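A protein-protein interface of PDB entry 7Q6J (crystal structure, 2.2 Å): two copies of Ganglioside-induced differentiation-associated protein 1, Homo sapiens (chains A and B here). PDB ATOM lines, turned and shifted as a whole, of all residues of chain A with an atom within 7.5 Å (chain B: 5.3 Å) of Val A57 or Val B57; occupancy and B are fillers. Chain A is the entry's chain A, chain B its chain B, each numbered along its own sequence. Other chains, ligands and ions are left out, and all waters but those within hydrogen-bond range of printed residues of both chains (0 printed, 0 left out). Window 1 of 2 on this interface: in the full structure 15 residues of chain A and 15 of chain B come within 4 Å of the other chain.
Among the printed residues, merely in contact across the chains: Ile A64 with Val B55 (3.4 Å), Trp A9 with Ile B64 (3.5 Å), Val A55 with Ile B64 (3.5 Å), Ile A64 with Tyr B7 (3.6 Å), Tyr A7 with Ile B64 (3.8 Å), Val A57 with Ile B64 (3.8 Å), Tyr A7 with Ile B59 (3.8 Å), Ile A64 with Val B57 (3.8 Å), His A8 with Ile B64 (3.9 Å), Ile A59 with Tyr B7 (3.9 Å) and Val A57 with Val B57 (3.96 Å).
Ile A5 touches none of the printed residues of chain B. Of chain B, only Val B57 and Ile B64 come within 4 Å of Val A57. Of the printed residues of chain B, Ile A59 touches Tyr B7. Printed residues of chain B within 4 Å of Cys A66: Cys B66 (2.1 Å). Pro B56 touches none of the printed residues of chain A. Val B57 touches just these residues of chain A: Val A57 and Ile A64. The nearest printed residue of chain B that does not touch Val A57 is Cys B66 (4.8 Å). The nearest residue of chain A that does not touch Val B57 is Cys A66 (4.5 Å).
Hydrophobic or aromatic side chains of chain A that line the printed part of chain B: Tyr A7, Trp A9, Val A55, Val A57, Ile A59 and Ile A64. Along chain A the printed residues that touch a printed residue of chain B span positions 7 to 66. Among the printed residues, 13 pairs touch across the chains.
Tyr A7 touches Ile B59, and with the chains exchanged Ile A59 touches Tyr B7. Val A55 touches Ile B64, and with the chains exchanged Ile A64 touches Val B55. Val A57 touches its own counterpart, Val B57. Val A57 touches Ile B64, and with the chains exchanged Ile A64 touches Val B57. 13 positions are printed for both chains. Of the 13 pairs that touch across the chains among the printed residues, 11 have their exchanged pair printed and touching as well.
The backbone NH (N) of Tyr A7 is in hydrogen-bond range of the backbone carbonyl oxygen (O) of Val A57. The backbone carbonyl oxygen (O) of His A32 lies within hydrogen-bond range of the backbone NH (N) of His A8 (3.0 Å). The backbone NH (N) of Ile A59 lies within hydrogen-bond range of the backbone carbonyl oxygen (O) of Ile A5 (2.8 Å). N of Tyr B7 is in hydrogen-bond range of O of Val B57 (3.1 Å). The backbone NH of Ile B59 is in hydrogen-bond range of the backbone carbonyl oxygen of Ile B5 (2.9 Å).
The side-chain sulfur (SG) of Cys A66 forms a disulfide with the side-chain sulfur (SG) of Cys B66. The side-chain hydroxyl (OH) of Tyr A7 is in hydrogen-bond range of the side-chain hydroxyl (OH) of Tyr B7, 2.7 Å away.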
ATOM      1  N   ILE A   5       4.935  17.946  -0.122  1.00  0.00           N
ATOM      2  CA  ILE A   5       4.126  18.975   0.518  1.00  0.00           C
ATOM      3  C   ILE A   5       3.371  18.298   1.649  1.00  0.00           C
ATOM      4  O   ILE A   5       2.754  17.248   1.433  1.00  0.00           O
ATOM      5  CB  ILE A   5       3.122  19.608  -0.463  1.00  0.00           C
ATOM      6  CG1 ILE A   5       3.806  20.237  -1.676  1.00  0.00           C
ATOM      7  CG2 ILE A   5       2.270  20.632   0.264  1.00  0.00           C
ATOM      8  CD1 ILE A   5       2.796  20.621  -2.782  1.00  0.00           C
ATOM      9  N   LEU A   6       3.437  18.883   2.855  1.00  0.00           N
ATOM     10  CA  LEU A   6       2.722  18.398   4.024  1.00  0.00           C
ATOM     11  C   LEU A   6       1.870  19.521   4.588  1.00  0.00           C
ATOM     12  O   LEU A   6       2.374  20.620   4.841  1.00  0.00           O
ATOM     13  CB  LEU A   6       3.700  17.900   5.100  1.00  0.00           C
ATOM     14  CG  LEU A   6       3.156  17.473   6.459  1.00  0.00           C
ATOM     15  CD1 LEU A   6       2.433  16.151   6.331  1.00  0.00           C
ATOM     16  CD2 LEU A   6       4.282  17.380   7.518  1.00  0.00           C
ATOM     17  N   TYR A   7       0.599  19.230   4.817  1.00  0.00           N
ATOM     18  CA  TYR A   7      -0.273  20.104   5.594  1.00  0.00           C
ATOM     19  C   TYR A   7      -0.563  19.415   6.907  1.00  0.00           C
ATOM     20  O   TYR A   7      -0.870  18.218   6.922  1.00  0.00           O
ATOM     21  CB  TYR A   7      -1.610  20.362   4.894  1.00  0.00           C
ATOM     22  CG  TYR A   7      -1.481  21.162   3.635  1.00  0.00           C
ATOM     23  CD1 TYR A   7      -1.568  22.541   3.670  1.00  0.00           C
ATOM     24  CD2 TYR A   7      -1.284  20.546   2.419  1.00  0.00           C
ATOM     25  CE1 TYR A   7      -1.456  23.291   2.522  1.00  0.00           C
ATOM     26  CE2 TYR A   7      -1.190  21.285   1.245  1.00  0.00           C
ATOM     27  CZ  TYR A   7      -1.280  22.653   1.307  1.00  0.00           C
ATOM     28  OH  TYR A   7      -1.146  23.398   0.166  1.00  0.00           O
ATOM     29  N   HIS A   8      -0.516  20.166   8.006  1.00  0.00           N
ATOM     30  CA  HIS A   8      -0.543  19.535   9.310  1.00  0.00           C
ATOM     31  C   HIS A   8      -0.782  20.611  10.356  1.00  0.00           C
ATOM     32  O   HIS A   8      -0.768  21.813  10.052  1.00  0.00           O
ATOM     33  CB  HIS A   8       0.786  18.833   9.564  1.00  0.00           C
ATOM     34  CG  HIS A   8       1.878  19.809   9.852  1.00  0.00           C
ATOM     35  ND1 HIS A   8       2.287  20.106  11.132  1.00  0.00           N
ATOM     36  CD2 HIS A   8       2.552  20.653   9.033  1.00  0.00           C
ATOM     37  CE1 HIS A   8       3.193  21.067  11.089  1.00  0.00           C
ATOM     38  NE2 HIS A   8       3.397  21.390   9.825  1.00  0.00           N
ATOM     39  N   TRP A   9      -0.962  20.162  11.599  1.00  0.00           N
ATOM     40  CA  TRP A   9      -0.980  21.054  12.747  1.00  0.00           C
ATOM     41  C   TRP A   9       0.191  20.715  13.655  1.00  0.00           C
ATOM     42  O   TRP A   9       0.286  19.594  14.167  1.00  0.00           O
ATOM     43  CB  TRP A   9      -2.261  20.940  13.552  1.00  0.00           C
ATOM     44  CG  TRP A   9      -3.450  20.978  12.773  1.00  0.00           C
ATOM     45  CD1 TRP A   9      -4.270  22.051  12.602  1.00  0.00           C
ATOM     46  CD2 TRP A   9      -4.021  19.897  12.039  1.00  0.00           C
ATOM     47  NE1 TRP A   9      -5.334  21.703  11.810  1.00  0.00           N
ATOM     48  CE2 TRP A   9      -5.207  20.384  11.447  1.00  0.00           C
ATOM     49  CE3 TRP A   9      -3.643  18.572  11.810  1.00  0.00           C
ATOM     50  CZ2 TRP A   9      -6.019  19.589  10.637  1.00  0.00           C
ATOM     51  CZ3 TRP A   9      -4.430  17.802  10.989  1.00  0.00           C
ATOM     52  CH2 TRP A   9      -5.610  18.303  10.423  1.00  0.00           C
ATOM     53  N   VAL A  18       4.861  12.274  11.943  1.00  0.00           N
ATOM     54  CA  VAL A  18       5.199  12.483  10.532  1.00  0.00           C
ATOM     55  C   VAL A  18       6.430  13.365  10.382  1.00  0.00           C
ATOM     56  O   VAL A  18       7.314  13.096   9.558  1.00  0.00           O
ATOM     57  CB  VAL A  18       4.020  13.102   9.767  1.00  0.00           C
ATOM     58  CG1 VAL A  18       4.488  13.421   8.356  1.00  0.00           C
ATOM     59  CG2 VAL A  18       2.857  12.178   9.792  1.00  0.00           C
ATOM     60  N   CYS A  29      11.030  18.832   2.537  1.00  0.00           N
ATOM     61  CA  CYS A  29       9.575  18.905   2.550  1.00  0.00           C
ATOM     62  C   CYS A  29       9.106  20.328   2.822  1.00  0.00           C
ATOM     63  O   CYS A  29       9.637  21.015   3.694  1.00  0.00           O
ATOM     64  CB  CYS A  29       8.976  17.972   3.612  1.00  0.00           C
ATOM     65  SG  CYS A  29       7.079  17.850   3.614  1.00  0.00           S
ATOM     66  N   GLU A  30       8.093  20.755   2.066  1.00  0.00           N
ATOM     67  CA  GLU A  30       7.423  22.049   2.234  1.00  0.00           C
ATOM     68  C   GLU A  30       6.258  21.836   3.191  1.00  0.00           C
ATOM     69  O   GLU A  30       5.243  21.254   2.813  1.00  0.00           O
ATOM     70  CB  GLU A  30       6.975  22.553   0.864  1.00  0.00           C
ATOM     71  CG  GLU A  30       6.183  23.840   0.787  1.00  0.00           C
ATOM     72  CD  GLU A  30       5.775  24.145  -0.670  1.00  0.00           C
ATOM     73  OE1 GLU A  30       4.564  24.261  -0.966  1.00  0.00           O
ATOM     74  OE2 GLU A  30       6.679  24.225  -1.535  1.00  0.00           O
ATOM     75  N   HIS A  32       3.285  22.937   5.781  1.00  0.00           N
ATOM     76  CA  HIS A  32       2.334  24.014   6.075  1.00  0.00           C
ATOM     77  C   HIS A  32       1.687  23.703   7.413  1.00  0.00           C
ATOM     78  O   HIS A  32       0.908  22.749   7.520  1.00  0.00           O
ATOM     79  CB  HIS A  32       1.262  24.162   4.999  1.00  0.00           C
ATOM     80  CG  HIS A  32       1.842  24.485   3.668  1.00  0.00           C
ATOM     81  ND1 HIS A  32       2.337  25.732   3.358  1.00  0.00           N
ATOM     82  CD2 HIS A  32       2.092  23.704   2.596  1.00  0.00           C
ATOM     83  CE1 HIS A  32       2.844  25.711   2.140  1.00  0.00           C
ATOM     84  NE2 HIS A  32       2.706  24.493   1.657  1.00  0.00           N
ATOM     85  N   VAL A  55      -5.927  15.384  11.078  1.00  0.00           N
ATOM     86  CA  VAL A  55      -5.322  14.402  10.177  1.00  0.00           C
ATOM     87  C   VAL A  55      -4.433  15.122   9.178  1.00  0.00           C
ATOM     88  O   VAL A  55      -4.918  15.915   8.365  1.00  0.00           O
ATOM     89  CB  VAL A  55      -6.366  13.591   9.421  1.00  0.00           C
ATOM     90  CG1 VAL A  55      -6.909  12.503  10.301  1.00  0.00           C
ATOM     91  CG2 VAL A  55      -7.482  14.517   8.992  1.00  0.00           C
ATOM     92  N   PRO A  56      -3.132  14.904   9.218  1.00  0.00           N
ATOM     93  CA  PRO A  56      -2.253  15.526   8.233  1.00  0.00           C
ATOM     94  C   PRO A  56      -2.412  14.900   6.863  1.00  0.00           C
ATOM     95  O   PRO A  56      -2.902  13.786   6.709  1.00  0.00           O
ATOM     96  CB  PRO A  56      -0.863  15.263   8.786  1.00  0.00           C
ATOM     97  CG  PRO A  56      -1.027  14.007   9.621  1.00  0.00           C
ATOM     98  CD  PRO A  56      -2.390  14.085  10.202  1.00  0.00           C
ATOM     99  N   VAL A  57      -1.888  15.594   5.860  1.00  0.00           N
ATOM    100  CA  VAL A  57      -1.968  15.119   4.491  1.00  0.00           C
ATOM    101  C   VAL A  57      -0.660  15.436   3.791  1.00  0.00           C
ATOM    102  O   VAL A  57      -0.125  16.546   3.913  1.00  0.00           O
ATOM    103  CB  VAL A  57      -3.155  15.762   3.753  1.00  0.00           C
ATOM    104  CG1 VAL A  57      -2.981  17.238   3.674  1.00  0.00           C
ATOM    105  CG2 VAL A  57      -3.234  15.258   2.341  1.00  0.00           C
ATOM    106  N   LEU A  58      -0.153  14.443   3.048  1.00  0.00           N
ATOM    107  CA  LEU A  58       1.030  14.585   2.219  1.00  0.00           C
ATOM    108  C   LEU A  58       0.589  14.545   0.758  1.00  0.00           C
ATOM    109  O   LEU A  58      -0.227  13.703   0.370  1.00  0.00           O
ATOM    110  CB  LEU A  58       2.021  13.463   2.504  1.00  0.00           C
ATOM    111  CG  LEU A  58       3.339  13.583   1.753  1.00  0.00           C
ATOM    112  CD1 LEU A  58       4.319  14.482   2.454  1.00  0.00           C
ATOM    113  CD2 LEU A  58       3.958  12.228   1.588  1.00  0.00           C
ATOM    114  N   ILE A  59       1.128  15.467  -0.024  1.00  0.00           N
ATOM    115  CA  ILE A  59       1.014  15.475  -1.467  1.00  0.00           C
ATOM    116  C   ILE A  59       2.401  15.279  -2.035  1.00  0.00           C
ATOM    117  O   ILE A  59       3.340  15.994  -1.661  1.00  0.00           O
ATOM    118  CB  ILE A  59       0.412  16.797  -1.947  1.00  0.00           C
ATOM    119  CG1 ILE A  59      -1.019  16.991  -1.367  1.00  0.00           C
ATOM    120  CG2 ILE A  59       0.318  16.809  -3.437  1.00  0.00           C
ATOM    121  CD1 ILE A  59      -1.077  18.081  -0.449  1.00  0.00           C
ATOM    122  N   ASN A  63       0.394  11.619  -5.911  1.00  0.00           N
ATOM    123  CA  ASN A  63      -0.126  10.897  -4.748  1.00  0.00           C
ATOM    124  C   ASN A  63      -0.619  11.840  -3.645  1.00  0.00           C
ATOM    125  O   ASN A  63      -0.003  12.870  -3.360  1.00  0.00           O
ATOM    126  CB  ASN A  63       0.970   9.977  -4.208  1.00  0.00           C
ATOM    127  CG  ASN A  63       1.313   8.882  -5.178  1.00  0.00           C
ATOM    128  OD1 ASN A  63       2.408   8.851  -5.755  1.00  0.00           O
ATOM    129  ND2 ASN A  63       0.404   7.931  -5.317  1.00  0.00           N
ATOM    130  N   ILE A  64      -1.726  11.464  -3.025  1.00  0.00           N
ATOM    131  CA  ILE A  64      -2.341  12.184  -1.913  1.00  0.00           C
ATOM    132  C   ILE A  64      -2.577  11.142  -0.839  1.00  0.00           C
ATOM    133  O   ILE A  64      -3.183  10.106  -1.106  1.00  0.00           O
ATOM    134  CB  ILE A  64      -3.663  12.852  -2.321  1.00  0.00           C
ATOM    135  CG1 ILE A  64      -3.412  13.867  -3.446  1.00  0.00           C
ATOM    136  CG2 ILE A  64      -4.290  13.577  -1.147  1.00  0.00           C
ATOM    137  CD1 ILE A  64      -4.704  14.517  -4.071  1.00  0.00           C
ATOM    138  N   ILE A  65      -1.976  11.331   0.311  1.00  0.00           N
ATOM    139  CA  ILE A  65      -2.050  10.354   1.381  1.00  0.00           C
ATOM    140  C   ILE A  65      -2.404  11.099   2.654  1.00  0.00           C
ATOM    141  O   ILE A  65      -1.708  12.061   3.019  1.00  0.00           O
ATOM    142  CB  ILE A  65      -0.702   9.612   1.571  1.00  0.00           C
ATOM    143  CG1 ILE A  65      -0.208   9.039   0.247  1.00  0.00           C
ATOM    144  CG2 ILE A  65      -0.849   8.467   2.527  1.00  0.00           C
ATOM    145  CD1 ILE A  65       0.653   9.995  -0.477  1.00  0.00           C
ATOM    146  N   CYS A  66      -3.443  10.629   3.346  1.00  0.00           N
ATOM    147  CA  CYS A  66      -3.923  11.216   4.591  1.00  0.00           C
ATOM    148  C   CYS A  66      -3.587  10.281   5.745  1.00  0.00           C
ATOM    149  O   CYS A  66      -3.480   9.070   5.555  1.00  0.00           O
ATOM    150  CB  CYS A  66      -5.458  11.440   4.545  1.00  0.00           C
ATOM    151  SG  CYS A  66      -6.023  12.492   3.123  1.00  0.00           S
ATOM    152  N   GLU A  67      -3.415  10.859   6.937  1.00  0.00           N
ATOM    153  CA  GLU A  67      -3.215  10.120   8.192  1.00  0.00           C
ATOM    154  C   GLU A  67      -1.791   9.678   8.371  1.00  0.00           C
ATOM    155  O   GLU A  67      -1.122   9.285   7.406  1.00  0.00           O
ATOM    156  CB  GLU A  67      -4.105   8.884   8.297  1.00  0.00           C
ATOM    157  CG  GLU A  67      -5.559   9.148   7.982  1.00  0.00           C
ATOM    158  CD  GLU A  67      -6.488   7.975   8.294  1.00  0.00           C
ATOM    159  OE1 GLU A  67      -7.392   8.152   9.146  1.00  0.00           O
ATOM    160  OE2 GLU A  67      -6.329   6.889   7.671  1.00  0.00           O
ATOM    161  N   ALA A  68      -1.345   9.703   9.624  1.00  0.00           N
ATOM    162  CA  ALA A  68       0.060   9.569   9.945  1.00  0.00           C
ATOM    163  C   ALA A  68       0.619   8.216   9.550  1.00  0.00           C
ATOM    164  O   ALA A  68       1.670   8.125   8.901  1.00  0.00           O
ATOM    165  CB  ALA A  68       0.203   9.809  11.442  1.00  0.00           C
ATOM    166  N   ILE A  71       0.870   7.934   5.753  1.00  0.00           N
ATOM    167  CA  ILE A  71       1.895   8.820   5.218  1.00  0.00           C
ATOM    168  C   ILE A  71       3.280   8.266   5.530  1.00  0.00           C
ATOM    169  O   ILE A  71       4.184   8.259   4.682  1.00  0.00           O
ATOM    170  CB  ILE A  71       1.732  10.233   5.805  1.00  0.00           C
ATOM    171  CG1 ILE A  71       0.473  10.936   5.333  1.00  0.00           C
ATOM    172  CG2 ILE A  71       3.002  11.024   5.574  1.00  0.00           C
ATOM    173  CD1 ILE A  71       0.262  12.256   6.066  1.00  0.00           C
ATOM    174  N   ILE B   5      -8.546  25.417  -0.731  1.00  0.00           N
ATOM    175  CA  ILE B   5      -7.581  24.702  -1.559  1.00  0.00           C
ATOM    176  C   ILE B   5      -8.045  23.269  -1.724  1.00  0.00           C
ATOM    177  O   ILE B   5      -8.313  22.594  -0.724  1.00  0.00           O
ATOM    178  CB  ILE B   5      -6.176  24.720  -0.922  1.00  0.00           C
ATOM    179  CG1 ILE B   5      -5.720  26.168  -0.728  1.00  0.00           C
ATOM    180  CG2 ILE B   5      -5.253  23.914  -1.758  1.00  0.00           C
ATOM    181  CD1 ILE B   5      -4.474  26.300   0.112  1.00  0.00           C
ATOM    182  N   LEU B   6      -8.065  22.779  -2.972  1.00  0.00           N
ATOM    183  CA  LEU B   6      -8.394  21.381  -3.239  1.00  0.00           C
ATOM    184  C   LEU B   6      -7.265  20.710  -4.022  1.00  0.00           C
ATOM    185  O   LEU B   6      -6.775  21.252  -5.018  1.00  0.00           O
ATOM    186  CB  LEU B   6      -9.727  21.270  -4.009  1.00  0.00           C
ATOM    187  CG  LEU B   6     -10.162  19.886  -4.494  1.00  0.00           C
ATOM    188  CD1 LEU B   6     -10.668  19.056  -3.347  1.00  0.00           C
ATOM    189  CD2 LEU B   6     -11.251  19.962  -5.597  1.00  0.00           C
ATOM    190  N   TYR B   7      -6.872  19.524  -3.578  1.00  0.00           N
ATOM    191  CA  TYR B   7      -5.996  18.640  -4.321  1.00  0.00           C
ATOM    192  C   TYR B   7      -6.797  17.421  -4.739  1.00  0.00           C
ATOM    193  O   TYR B   7      -7.468  16.797  -3.904  1.00  0.00           O
ATOM    194  CB  TYR B   7      -4.814  18.223  -3.438  1.00  0.00           C
ATOM    195  CG  TYR B   7      -3.823  19.333  -3.162  1.00  0.00           C
ATOM    196  CD1 TYR B   7      -2.727  19.540  -4.001  1.00  0.00           C
ATOM    197  CD2 TYR B   7      -3.966  20.172  -2.061  1.00  0.00           C
ATOM    198  CE1 TYR B   7      -1.784  20.550  -3.732  1.00  0.00           C
ATOM    199  CE2 TYR B   7      -3.028  21.187  -1.789  1.00  0.00           C
ATOM    200  CZ  TYR B   7      -1.938  21.360  -2.619  1.00  0.00           C
ATOM    201  OH  TYR B   7      -1.003  22.351  -2.369  1.00  0.00           O
ATOM    202  N   VAL B  55      -7.782   9.429  -1.807  1.00  0.00           N
ATOM    203  CA  VAL B  55      -8.913  10.348  -1.829  1.00  0.00           C
ATOM    204  C   VAL B  55      -8.494  11.800  -2.057  1.00  0.00           C
ATOM    205  O   VAL B  55      -7.352  12.162  -1.781  1.00  0.00           O
ATOM    206  CB  VAL B  55      -9.721  10.170  -0.533  1.00  0.00           C
ATOM    207  CG1 VAL B  55     -10.520   8.845  -0.603  1.00  0.00           C
ATOM    208  CG2 VAL B  55      -8.800  10.214   0.707  1.00  0.00           C
ATOM    209  N   PRO B  56      -9.359  12.644  -2.615  1.00  0.00           N
ATOM    210  CA  PRO B  56      -9.060  14.077  -2.662  1.00  0.00           C
ATOM    211  C   PRO B  56      -9.048  14.667  -1.254  1.00  0.00           C
ATOM    212  O   PRO B  56      -9.530  14.078  -0.283  1.00  0.00           O
ATOM    213  CB  PRO B  56     -10.229  14.664  -3.464  1.00  0.00           C
ATOM    214  CG  PRO B  56     -11.356  13.741  -3.192  1.00  0.00           C
ATOM    215  CD  PRO B  56     -10.735  12.359  -3.062  1.00  0.00           C
ATOM    216  N   VAL B  57      -8.539  15.890  -1.152  1.00  0.00           N
ATOM    217  CA  VAL B  57      -8.410  16.531   0.157  1.00  0.00           C
ATOM    218  C   VAL B  57      -8.656  18.015  -0.008  1.00  0.00           C
ATOM    219  O   VAL B  57      -8.204  18.622  -0.982  1.00  0.00           O
ATOM    220  CB  VAL B  57      -7.019  16.274   0.788  1.00  0.00           C
ATOM    221  CG1 VAL B  57      -5.943  16.868  -0.054  1.00  0.00           C
ATOM    222  CG2 VAL B  57      -6.900  16.858   2.257  1.00  0.00           C
ATOM    223  N   LEU B  58      -9.375  18.587   0.946  1.00  0.00           N
ATOM    224  CA  LEU B  58      -9.615  20.015   1.024  1.00  0.00           C
ATOM    225  C   LEU B  58      -8.867  20.600   2.206  1.00  0.00           C
ATOM    226  O   LEU B  58      -8.878  20.021   3.291  1.00  0.00           O
ATOM    227  CB  LEU B  58     -11.104  20.293   1.257  1.00  0.00           C
ATOM    228  CG  LEU B  58     -11.528  21.752   1.249  1.00  0.00           C
ATOM    229  CD1 LEU B  58     -11.619  22.169  -0.189  1.00  0.00           C
ATOM    230  CD2 LEU B  58     -12.902  21.928   1.903  1.00  0.00           C
ATOM    231  N   ILE B  59      -8.260  21.764   2.005  1.00  0.00           N
ATOM    232  CA  ILE B  59      -7.683  22.553   3.076  1.00  0.00           C
ATOM    233  C   ILE B  59      -8.417  23.888   3.134  1.00  0.00           C
ATOM    234  O   ILE B  59      -8.511  24.593   2.120  1.00  0.00           O
ATOM    235  CB  ILE B  59      -6.173  22.761   2.862  1.00  0.00           C
ATOM    236  CG1 ILE B  59      -5.411  21.422   2.930  1.00  0.00           C
ATOM    237  CG2 ILE B  59      -5.634  23.765   3.865  1.00  0.00           C
ATOM    238  CD1 ILE B  59      -4.974  21.031   1.538  1.00  0.00           C
ATOM    239  N   ILE B  64      -8.573  20.300   7.586  1.00  0.00           N
ATOM    240  CA  ILE B  64      -8.062  19.422   6.532  1.00  0.00           C
ATOM    241  C   ILE B  64      -9.052  18.286   6.440  1.00  0.00           C
ATOM    242  O   ILE B  64      -9.254  17.572   7.423  1.00  0.00           O
ATOM    243  CB  ILE B  64      -6.668  18.878   6.860  1.00  0.00           C
ATOM    244  CG1 ILE B  64      -5.692  20.044   7.024  1.00  0.00           C
ATOM    245  CG2 ILE B  64      -6.088  17.895   5.722  1.00  0.00           C
ATOM    246  CD1 ILE B  64      -4.310  19.642   7.487  1.00  0.00           C
ATOM    247  N   ILE B  65      -9.679  18.127   5.287  1.00  0.00           N
ATOM    248  CA  ILE B  65     -10.736  17.134   5.113  1.00  0.00           C
ATOM    249  C   ILE B  65     -10.423  16.303   3.875  1.00  0.00           C
ATOM    250  O   ILE B  65     -10.170  16.845   2.790  1.00  0.00           O
ATOM    251  CB  ILE B  65     -12.123  17.795   4.998  1.00  0.00           C
ATOM    252  CG1 ILE B  65     -12.330  18.769   6.149  1.00  0.00           C
ATOM    253  CG2 ILE B  65     -13.282  16.765   5.089  1.00  0.00           C
ATOM    254  CD1 ILE B  65     -11.905  20.140   5.808  1.00  0.00           C
ATOM    255  N   CYS B  66     -10.398  14.990   4.077  1.00  0.00           N
ATOM    256  CA  CYS B  66     -10.174  13.958   3.104  1.00  0.00           C
ATOM    257  C   CYS B  66     -11.471  13.204   2.797  1.00  0.00           C
ATOM    258  O   CYS B  66     -12.342  13.052   3.656  1.00  0.00           O
ATOM    259  CB  CYS B  66      -9.115  12.985   3.653  1.00  0.00           C
ATOM    260  SG  CYS B  66      -7.479  13.760   4.032  1.00  0.00           S
ATOM    261  N   GLU B  67     -11.538  12.670   1.569  1.00  0.00           N
ATOM    262  CA  GLU B  67     -12.615  11.836   1.037  1.00  0.00           C
ATOM    263  C   GLU B  67     -13.770  12.720   0.583  1.00  0.00           C
ATOM    264  O   GLU B  67     -14.127  13.716   1.227  1.00  0.00           O
ATOM    265  CB  GLU B  67     -13.090  10.781   2.035  1.00  0.00           C
ATOM    266  CG  GLU B  67     -11.942  10.013   2.676  1.00  0.00           C
ATOM    267  CD  GLU B  67     -12.361   8.717   3.404  1.00  0.00           C
ATOM    268  OE1 GLU B  67     -11.847   7.641   2.998  1.00  0.00           O
ATOM    269  OE2 GLU B  67     -13.161   8.771   4.379  1.00  0.00           O
ATOM    270  N   ILE B  71     -15.672  15.930   2.437  1.00  0.00           N
ATOM    271  CA  ILE B  71     -15.422  17.278   1.931  1.00  0.00           C
ATOM    272  C   ILE B  71     -16.758  17.947   1.602  1.00  0.00           C
ATOM    273  O   ILE B  71     -16.995  19.119   1.926  1.00  0.00           O
ATOM    274  CB  ILE B  71     -14.518  17.234   0.688  1.00  0.00           C
ATOM    275  CG1 ILE B  71     -13.120  16.733   1.026  1.00  0.00           C
ATOM    276  CG2 ILE B  71     -14.543  18.617   0.013  1.00  0.00           C
ATOM    277  CD1 ILE B  71     -12.287  16.449  -0.227  1.00  0.00           C
